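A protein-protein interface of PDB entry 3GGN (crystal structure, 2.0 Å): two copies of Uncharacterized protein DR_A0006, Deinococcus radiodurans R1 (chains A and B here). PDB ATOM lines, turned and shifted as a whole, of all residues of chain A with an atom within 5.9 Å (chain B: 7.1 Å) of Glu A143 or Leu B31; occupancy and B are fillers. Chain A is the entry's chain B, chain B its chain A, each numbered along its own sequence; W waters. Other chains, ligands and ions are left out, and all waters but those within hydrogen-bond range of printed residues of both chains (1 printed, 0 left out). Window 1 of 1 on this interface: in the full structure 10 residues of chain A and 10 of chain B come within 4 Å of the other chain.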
ATOM      1  N   MET A 138      15.501 -24.413 -20.674  1.00  0.00           N
ATOM      2  CA  MET A 138      14.904 -23.176 -21.168  1.00  0.00           C
ATOM      3  C   MET A 138      13.485 -23.439 -21.684  1.00  0.00           C
ATOM      4  O   MET A 138      12.571 -22.641 -21.456  1.00  0.00           O
ATOM      5  CB  MET A 138      15.779 -22.560 -22.265  1.00  0.00           C
ATOM      6  CG  MET A 138      17.087 -21.985 -21.743  1.00  0.00           C
ATOM      7  SD  MET A 138      18.165 -21.341 -23.046  1.00  0.00           S
ATOM      8  CE  MET A 138      17.756 -19.597 -22.991  1.00  0.00           C
ATOM      9  N   ARG A 139      13.289 -24.560 -22.371  1.00  0.00           N
ATOM     10  CA  ARG A 139      11.957 -24.873 -22.861  1.00  0.00           C
ATOM     11  C   ARG A 139      11.022 -25.111 -21.676  1.00  0.00           C
ATOM     12  O   ARG A 139       9.873 -24.665 -21.681  1.00  0.00           O
ATOM     13  CB  ARG A 139      11.996 -26.092 -23.793  1.00  0.00           C
ATOM     14  CG  ARG A 139      12.658 -25.762 -25.135  1.00  0.00           C
ATOM     15  CD  ARG A 139      12.470 -26.831 -26.211  1.00  0.00           C
ATOM     16  NE  ARG A 139      13.268 -28.026 -25.960  1.00  0.00           N
ATOM     17  CZ  ARG A 139      12.834 -29.078 -25.276  1.00  0.00           C
ATOM     18  NH1 ARG A 139      11.601 -29.082 -24.785  1.00  0.00           N
ATOM     19  NH2 ARG A 139      13.635 -30.115 -25.070  1.00  0.00           N
ATOM     20  N   PHE A 140      11.525 -25.804 -20.660  1.00  0.00           N
ATOM     21  CA  PHE A 140      10.753 -26.084 -19.452  1.00  0.00           C
ATOM     22  C   PHE A 140      10.335 -24.766 -18.797  1.00  0.00           C
ATOM     23  O   PHE A 140       9.217 -24.634 -18.293  1.00  0.00           O
ATOM     24  CB  PHE A 140      11.599 -26.918 -18.479  1.00  0.00           C
ATOM     25  CG  PHE A 140      10.941 -27.163 -17.147  1.00  0.00           C
ATOM     26  CD1 PHE A 140       9.702 -27.796 -17.070  1.00  0.00           C
ATOM     27  CD2 PHE A 140      11.580 -26.791 -15.962  1.00  0.00           C
ATOM     28  CE1 PHE A 140       9.109 -28.059 -15.825  1.00  0.00           C
ATOM     29  CE2 PHE A 140      10.999 -27.049 -14.723  1.00  0.00           C
ATOM     30  CZ  PHE A 140       9.754 -27.688 -14.657  1.00  0.00           C
ATOM     31  N   LYS A 141      11.238 -23.789 -18.809  1.00  0.00           N
ATOM     32  CA  LYS A 141      10.955 -22.477 -18.236  1.00  0.00           C
ATOM     33  C   LYS A 141       9.841 -21.788 -19.030  1.00  0.00           C
ATOM     34  O   LYS A 141       8.844 -21.346 -18.471  1.00  0.00           O
ATOM     35  CB  LYS A 141      12.214 -21.611 -18.272  1.00  0.00           C
ATOM     36  CG  LYS A 141      11.997 -20.173 -17.821  1.00  0.00           C
ATOM     37  CD  LYS A 141      13.307 -19.400 -17.899  1.00  0.00           C
ATOM     38  CE  LYS A 141      13.185 -18.034 -17.246  1.00  0.00           C
ATOM     39  NZ  LYS A 141      12.101 -17.236 -17.854  1.00  0.00           N
ATOM     40  N   ARG A 142      10.024 -21.702 -20.343  1.00  0.00           N
ATOM     41  CA  ARG A 142       9.036 -21.071 -21.214  1.00  0.00           C
ATOM     42  C   ARG A 142       7.674 -21.733 -21.102  1.00  0.00           C
ATOM     43  O   ARG A 142       6.651 -21.056 -20.994  1.00  0.00           O
ATOM     44  CB  ARG A 142       9.509 -21.132 -22.669  1.00  0.00           C
ATOM     45  CG  ARG A 142       8.473 -20.694 -23.701  1.00  0.00           C
ATOM     46  CD  ARG A 142       9.049 -20.804 -25.109  1.00  0.00           C
ATOM     47  NE  ARG A 142       8.055 -20.503 -26.137  1.00  0.00           N
ATOM     48  CZ  ARG A 142       7.185 -21.384 -26.615  1.00  0.00           C
ATOM     49  NH1 ARG A 142       7.189 -22.638 -26.170  1.00  0.00           N
ATOM     50  NH2 ARG A 142       6.289 -21.001 -27.514  1.00  0.00           N
ATOM     51  N   GLU A 143       7.663 -23.061 -21.132  1.00  0.00           N
ATOM     52  CA  GLU A 143       6.421 -23.816 -21.052  1.00  0.00           C
ATOM     53  C   GLU A 143       5.679 -23.564 -19.753  1.00  0.00           C
ATOM     54  O   GLU A 143       4.465 -23.354 -19.752  1.00  0.00           O
ATOM     55  CB  GLU A 143       6.708 -25.308 -21.224  1.00  0.00           C
ATOM     56  CG  GLU A 143       7.065 -25.677 -22.657  1.00  0.00           C
ATOM     57  CD  GLU A 143       7.532 -27.112 -22.804  1.00  0.00           C
ATOM     58  OE1 GLU A 143       6.887 -28.014 -22.228  1.00  0.00           O
ATOM     59  OE2 GLU A 143       8.543 -27.333 -23.504  1.00  0.00           O
ATOM     60  N   GLN A 144       6.409 -23.585 -18.644  1.00  0.00           N
ATOM     61  CA  GLN A 144       5.803 -23.349 -17.345  1.00  0.00           C
ATOM     62  C   GLN A 144       5.315 -21.912 -17.192  1.00  0.00           C
ATOM     63  O   GLN A 144       4.190 -21.690 -16.753  1.00  0.00           O
ATOM     64  CB  GLN A 144       6.795 -23.677 -16.224  1.00  0.00           C
ATOM     65  CG  GLN A 144       6.994 -25.167 -15.996  1.00  0.00           C
ATOM     66  CD  GLN A 144       5.745 -25.845 -15.469  1.00  0.00           C
ATOM     67  OE1 GLN A 144       5.128 -25.373 -14.508  1.00  0.00           O
ATOM     68  NE2 GLN A 144       5.370 -26.958 -16.082  1.00  0.00           N
ATOM     69  N   GLU A 145       6.154 -20.943 -17.560  1.00  0.00           N
ATOM     70  CA  GLU A 145       5.789 -19.537 -17.432  1.00  0.00           C
ATOM     71  C   GLU A 145       4.646 -19.105 -18.347  1.00  0.00           C
ATOM     72  O   GLU A 145       3.988 -18.099 -18.080  1.00  0.00           O
ATOM     73  CB  GLU A 145       7.014 -18.641 -17.654  1.00  0.00           C
ATOM     74  CG  GLU A 145       8.191 -19.006 -16.746  1.00  0.00           C
ATOM     75  CD  GLU A 145       9.200 -17.891 -16.572  1.00  0.00           C
ATOM     76  OE1 GLU A 145       9.411 -17.111 -17.526  1.00  0.00           O
ATOM     77  OE2 GLU A 145       9.798 -17.810 -15.476  1.00  0.00           O
ATOM     78  N   LEU A 146       4.405 -19.856 -19.420  1.00  0.00           N
ATOM     79  CA  LEU A 146       3.313 -19.533 -20.336  1.00  0.00           C
ATOM     80  C   LEU A 146       2.064 -20.316 -19.956  1.00  0.00           C
ATOM     81  O   LEU A 146       0.943 -19.902 -20.253  1.00  0.00           O
ATOM     82  CB  LEU A 146       3.704 -19.850 -21.779  1.00  0.00           C
ATOM     83  CG  LEU A 146       4.781 -18.928 -22.364  1.00  0.00           C
ATOM     84  CD1 LEU A 146       5.163 -19.389 -23.757  1.00  0.00           C
ATOM     85  CD2 LEU A 146       4.253 -17.501 -22.392  1.00  0.00           C
ATOM     86  N   GLY A 147       2.263 -21.453 -19.297  1.00  0.00           N
ATOM     87  CA  GLY A 147       1.141 -22.265 -18.875  1.00  0.00           C
ATOM     88  C   GLY A 147       0.659 -23.301 -19.871  1.00  0.00           C
ATOM     89  O   GLY A 147      -0.357 -23.953 -19.633  1.00  0.00           O
ATOM     90  N   LEU A 148       1.369 -23.470 -20.984  1.00  0.00           N
ATOM     91  CA  LEU A 148       0.949 -24.456 -21.971  1.00  0.00           C
ATOM     92  C   LEU A 148       1.400 -25.864 -21.593  1.00  0.00           C
ATOM     93  O   LEU A 148       0.566 -26.793 -21.688  1.00  0.00           O
ATOM     94  CB  LEU A 148       1.458 -24.075 -23.370  1.00  0.00           C
ATOM     95  CG  LEU A 148       2.950 -23.813 -23.408  1.00  0.00           C
ATOM     96  CD1 LEU A 148       3.759 -24.710 -23.168  1.00  0.00           C
ATOM     97  CD2 LEU A 148       3.325 -22.571 -23.720  1.00  0.00           C
ATOM     98  N   LEU B  26      -5.695 -24.906 -31.251  1.00  0.00           N
ATOM     99  CA  LEU B  26      -4.912 -23.690 -31.445  1.00  0.00           C
ATOM    100  C   LEU B  26      -4.139 -23.136 -30.255  1.00  0.00           C
ATOM    101  O   LEU B  26      -2.997 -22.700 -30.413  1.00  0.00           O
ATOM    102  CB  LEU B  26      -5.808 -22.597 -32.035  1.00  0.00           C
ATOM    103  CG  LEU B  26      -6.532 -22.941 -33.340  1.00  0.00           C
ATOM    104  CD1 LEU B  26      -7.162 -21.675 -33.895  1.00  0.00           C
ATOM    105  CD2 LEU B  26      -5.568 -23.529 -34.354  1.00  0.00           C
ATOM    106  N   PRO B  27      -4.742 -23.135 -29.049  1.00  0.00           N
ATOM    107  CA  PRO B  27      -4.030 -22.610 -27.881  1.00  0.00           C
ATOM    108  C   PRO B  27      -2.735 -23.361 -27.606  1.00  0.00           C
ATOM    109  O   PRO B  27      -1.830 -22.845 -26.945  1.00  0.00           O
ATOM    110  CB  PRO B  27      -5.047 -22.768 -26.751  1.00  0.00           C
ATOM    111  CG  PRO B  27      -6.356 -22.672 -27.456  1.00  0.00           C
ATOM    112  CD  PRO B  27      -6.120 -23.511 -28.688  1.00  0.00           C
ATOM    113  N   GLY B  28      -2.644 -24.581 -28.120  1.00  0.00           N
ATOM    114  CA  GLY B  28      -1.445 -25.374 -27.916  1.00  0.00           C
ATOM    115  C   GLY B  28      -0.376 -25.200 -28.992  1.00  0.00           C
ATOM    116  O   GLY B  28       0.722 -25.739 -28.861  1.00  0.00           O
ATOM    117  N   LEU B  29      -0.677 -24.443 -30.046  1.00  0.00           N
ATOM    118  CA  LEU B  29       0.286 -24.251 -31.136  1.00  0.00           C
ATOM    119  C   LEU B  29       1.667 -23.735 -30.733  1.00  0.00           C
ATOM    120  O   LEU B  29       2.665 -24.112 -31.342  1.00  0.00           O
ATOM    121  CB  LEU B  29      -0.293 -23.327 -32.209  1.00  0.00           C
ATOM    122  CG  LEU B  29      -1.345 -23.961 -33.118  1.00  0.00           C
ATOM    123  CD1 LEU B  29      -1.805 -22.949 -34.166  1.00  0.00           C
ATOM    124  CD2 LEU B  29      -0.756 -25.181 -33.787  1.00  0.00           C
ATOM    125  N   PRO B  30       1.743 -22.851 -29.724  1.00  0.00           N
ATOM    126  CA  PRO B  30       3.051 -22.333 -29.305  1.00  0.00           C
ATOM    127  C   PRO B  30       4.010 -23.431 -28.834  1.00  0.00           C
ATOM    128  O   PRO B  30       5.205 -23.194 -28.687  1.00  0.00           O
ATOM    129  CB  PRO B  30       2.692 -21.356 -28.192  1.00  0.00           C
ATOM    130  CG  PRO B  30       1.367 -20.826 -28.651  1.00  0.00           C
ATOM    131  CD  PRO B  30       0.659 -22.103 -29.063  1.00  0.00           C
ATOM    132  N   LEU B  31       3.479 -24.620 -28.571  1.00  0.00           N
ATOM    133  CA  LEU B  31       4.317 -25.748 -28.162  1.00  0.00           C
ATOM    134  C   LEU B  31       4.941 -26.343 -29.419  1.00  0.00           C
ATOM    135  O   LEU B  31       6.110 -26.740 -29.429  1.00  0.00           O
ATOM    136  CB  LEU B  31       3.486 -26.828 -27.464  1.00  0.00           C
ATOM    137  CG  LEU B  31       3.455 -26.817 -25.936  1.00  0.00           C
ATOM    138  CD1 LEU B  31       2.555 -27.928 -25.435  1.00  0.00           C
ATOM    139  CD2 LEU B  31       4.870 -27.001 -25.394  1.00  0.00           C
ATOM    140  N   LEU B  32       4.150 -26.390 -30.485  1.00  0.00           N
ATOM    141  CA  LEU B  32       4.601 -26.945 -31.753  1.00  0.00           C
ATOM    142  C   LEU B  32       5.432 -25.952 -32.546  1.00  0.00           C
ATOM    143  O   LEU B  32       6.426 -26.329 -33.169  1.00  0.00           O
ATOM    144  CB  LEU B  32       3.398 -27.387 -32.586  1.00  0.00           C
ATOM    145  CG  LEU B  32       2.482 -28.443 -31.963  1.00  0.00           C
ATOM    146  CD1 LEU B  32       1.270 -28.640 -32.855  1.00  0.00           C
ATOM    147  CD2 LEU B  32       3.242 -29.754 -31.788  1.00  0.00           C
ATOM    148  N   MET B  33       5.013 -24.690 -32.543  1.00  0.00           N
ATOM    149  CA  MET B  33       5.734 -23.629 -33.252  1.00  0.00           C
ATOM    150  C   MET B  33       6.197 -22.652 -32.177  1.00  0.00           C
ATOM    151  O   MET B  33       5.555 -21.628 -31.924  1.00  0.00           O
ATOM    152  CB  MET B  33       4.813 -22.924 -34.258  1.00  0.00           C
ATOM    153  CG  MET B  33       4.183 -23.861 -35.293  1.00  0.00           C
ATOM    154  SD  MET B  33       3.242 -23.041 -36.620  1.00  0.00           S
ATOM    155  CE  MET B  33       4.111 -23.683 -37.984  1.00  0.00           C
ATOM    156  N   THR B  34       7.328 -22.976 -31.560  1.00  0.00           N
ATOM    157  CA  THR B  34       7.869 -22.183 -30.467  1.00  0.00           C
ATOM    158  C   THR B  34       8.194 -20.710 -30.714  1.00  0.00           C
ATOM    159  O   THR B  34       8.592 -20.015 -29.782  1.00  0.00           O
ATOM    160  CB  THR B  34       9.107 -22.870 -29.867  1.00  0.00           C
ATOM    161  OG1 THR B  34      10.135 -22.977 -30.860  1.00  0.00           O
ATOM    162  CG2 THR B  34       8.734 -24.263 -29.370  1.00  0.00           C
ATOM    163  N   LEU B  36       5.978 -18.761 -31.459  1.00  0.00           N
ATOM    164  CA  LEU B  36       4.716 -18.155 -31.037  1.00  0.00           C
ATOM    165  C   LEU B  36       4.645 -18.106 -29.514  1.00  0.00           C
ATOM    166  O   LEU B  36       5.095 -19.037 -28.839  1.00  0.00           O
ATOM    167  CB  LEU B  36       3.523 -18.968 -31.551  1.00  0.00           C
ATOM    168  CG  LEU B  36       3.154 -18.924 -33.032  1.00  0.00           C
ATOM    169  CD1 LEU B  36       1.974 -19.870 -33.287  1.00  0.00           C
ATOM    170  CD2 LEU B  36       2.792 -17.499 -33.434  1.00  0.00           C
ATOM    171  N   ASP B 136      11.499 -27.873 -33.920  1.00  0.00           N
ATOM    172  CA  ASP B 136      10.149 -28.006 -33.374  1.00  0.00           C
ATOM    173  C   ASP B 136       9.457 -29.272 -33.881  1.00  0.00           C
ATOM    174  O   ASP B 136       8.873 -30.020 -33.097  1.00  0.00           O
ATOM    175  CB  ASP B 136       9.299 -26.779 -33.733  1.00  0.00           C
ATOM    176  CG  ASP B 136       9.697 -25.539 -32.944  1.00  0.00           C
ATOM    177  OD1 ASP B 136      10.510 -25.667 -32.003  1.00  0.00           O
ATOM    178  OD2 ASP B 136       9.193 -24.437 -33.254  1.00  0.00           O
ATOM    179  N   ARG B 139      11.137 -32.494 -32.600  1.00  0.00           N
ATOM    180  CA  ARG B 139      10.729 -32.673 -31.210  1.00  0.00           C
ATOM    181  C   ARG B 139       9.313 -33.280 -31.200  1.00  0.00           C
ATOM    182  O   ARG B 139       9.049 -34.258 -30.491  1.00  0.00           O
ATOM    183  CB  ARG B 139      10.750 -31.320 -30.488  1.00  0.00           C
ATOM    184  CG  ARG B 139      10.710 -31.395 -28.966  1.00  0.00           C
ATOM    185  CD  ARG B 139      10.837 -30.000 -28.362  1.00  0.00           C
ATOM    186  NE  ARG B 139      12.008 -29.333 -28.909  1.00  0.00           N
ATOM    187  CZ  ARG B 139      11.989 -28.155 -29.525  1.00  0.00           C
ATOM    188  NH1 ARG B 139      10.853 -27.481 -29.668  1.00  0.00           N
ATOM    189  NH2 ARG B 139      13.109 -27.671 -30.036  1.00  0.00           N
ATOM    190  N   PHE B 140       8.414 -32.706 -31.999  1.00  0.00           N
ATOM    191  CA  PHE B 140       7.040 -33.198 -32.101  1.00  0.00           C
ATOM    192  C   PHE B 140       7.038 -34.669 -32.519  1.00  0.00           C
ATOM    193  O   PHE B 140       6.305 -35.496 -31.962  1.00  0.00           O
ATOM    194  CB  PHE B 140       6.265 -32.368 -33.136  1.00  0.00           C
ATOM    195  CG  PHE B 140       4.876 -32.885 -33.432  1.00  0.00           C
ATOM    196  CD1 PHE B 140       3.972 -33.134 -32.402  1.00  0.00           C
ATOM    197  CD2 PHE B 140       4.456 -33.072 -34.750  1.00  0.00           C
ATOM    198  CE1 PHE B 140       2.667 -33.557 -32.674  1.00  0.00           C
ATOM    199  CE2 PHE B 140       3.151 -33.494 -35.036  1.00  0.00           C
ATOM    200  CZ  PHE B 140       2.255 -33.737 -33.991  1.00  0.00           C
ATOM    201  N   GLU B 143       8.252 -36.891 -29.543  1.00  0.00           N
ATOM    202  CA  GLU B 143       7.252 -37.069 -28.500  1.00  0.00           C
ATOM    203  C   GLU B 143       6.185 -38.070 -28.922  1.00  0.00           C
ATOM    204  O   GLU B 143       5.907 -39.029 -28.201  1.00  0.00           O
ATOM    205  CB  GLU B 143       6.624 -35.719 -28.130  1.00  0.00           C
ATOM    206  CG  GLU B 143       7.589 -34.824 -27.361  1.00  0.00           C
ATOM    207  CD  GLU B 143       7.016 -33.458 -27.031  1.00  0.00           C
ATOM    208  OE1 GLU B 143       5.877 -33.396 -26.515  1.00  0.00           O
ATOM    209  OE2 GLU B 143       7.715 -32.448 -27.277  1.00  0.00           O
HETATM  210  O   HOH W   1      10.808 -20.059 -28.065  1.00  0.00           O
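Glu A143 touches just one residue of chain B: Leu B31 (3.7 Å).
Leu B31 touches two residues of chain A.
Of the printed residues of chain A, Leu B36 touches Arg A142 (2.7 Å).
Of the printed residues of chain B, Arg A139 touches Arg B139.
Printed residues of chain B within 4 Å of Leu A148: Leu B31 (3.4 Å).
The nearest residue of chain B that does not touch Glu A143 is Arg B139 (6.0 Å).
The nearest residue of chain A that does not touch Leu B31 is Arg A142 (4.7 Å).
The nearest printed residue of chain A that does not touch Thr B34 is Arg A139 (5.5 Å).
The side-chain carboxylate (OD2) of Asp B136 sits at hydrogen-bond distance from the backbone NH (N) of Thr B34 (2.9 Å).
The guanidinium group (NH1) of Arg B139 is in salt-bridge range of the side-chain carboxylate (OD1) of Asp B136.
NH1 of Arg A139 lies within salt-bridge range of OE2 of Glu A143, 3.7 Å away.
The backbone carbonyl oxygen (O) of Glu A143 lies within hydrogen-bond range of the backbone NH (N) of Leu A148 (3.3 Å).
Of the 11 printed residues of chain A, 4 touch a printed residue of chain B.
Hydrophobic or aromatic side chains of chain A that line the printed part of chain B: Leu A148.
Among the printed residues, 6 pairs touch across the chains.
Among the printed residues, no Asp or Glu carboxylate lies within 4 Å of a Lys or Arg side-chain nitrogen of the other chain.
Among the printed residues, pairs that only touch across the chains: Glu A143 with Leu B31 and Leu A148 with Leu B31.
The backbone carbonyl oxygen of Pro B30 sits at hydrogen-bond distance from the guanidinium group of Arg A142 (2.7 Å).
The backbone carbonyl oxygen (O) of Thr B34 lies within hydrogen-bond range of the guanidinium group (NH2) of Arg A142, 3.4 Å away.
NH2 of Arg A142 is in hydrogen-bond range of O of Leu B36 (2.7 Å).
The guanidinium group of Arg A139 sits close to the guanidinium group of Arg B139.
Water W1 lies within hydrogen-bond range of O of Thr B34 (2.8 Å) and NE of Arg A142 (3.4 Å).
Arg B139 touches its own counterpart, Arg A139.
3 positions are printed for both chains.
Of the 6 pairs that touch across the chains among the printed residues, 1 has its exchanged pair printed and touching as well.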
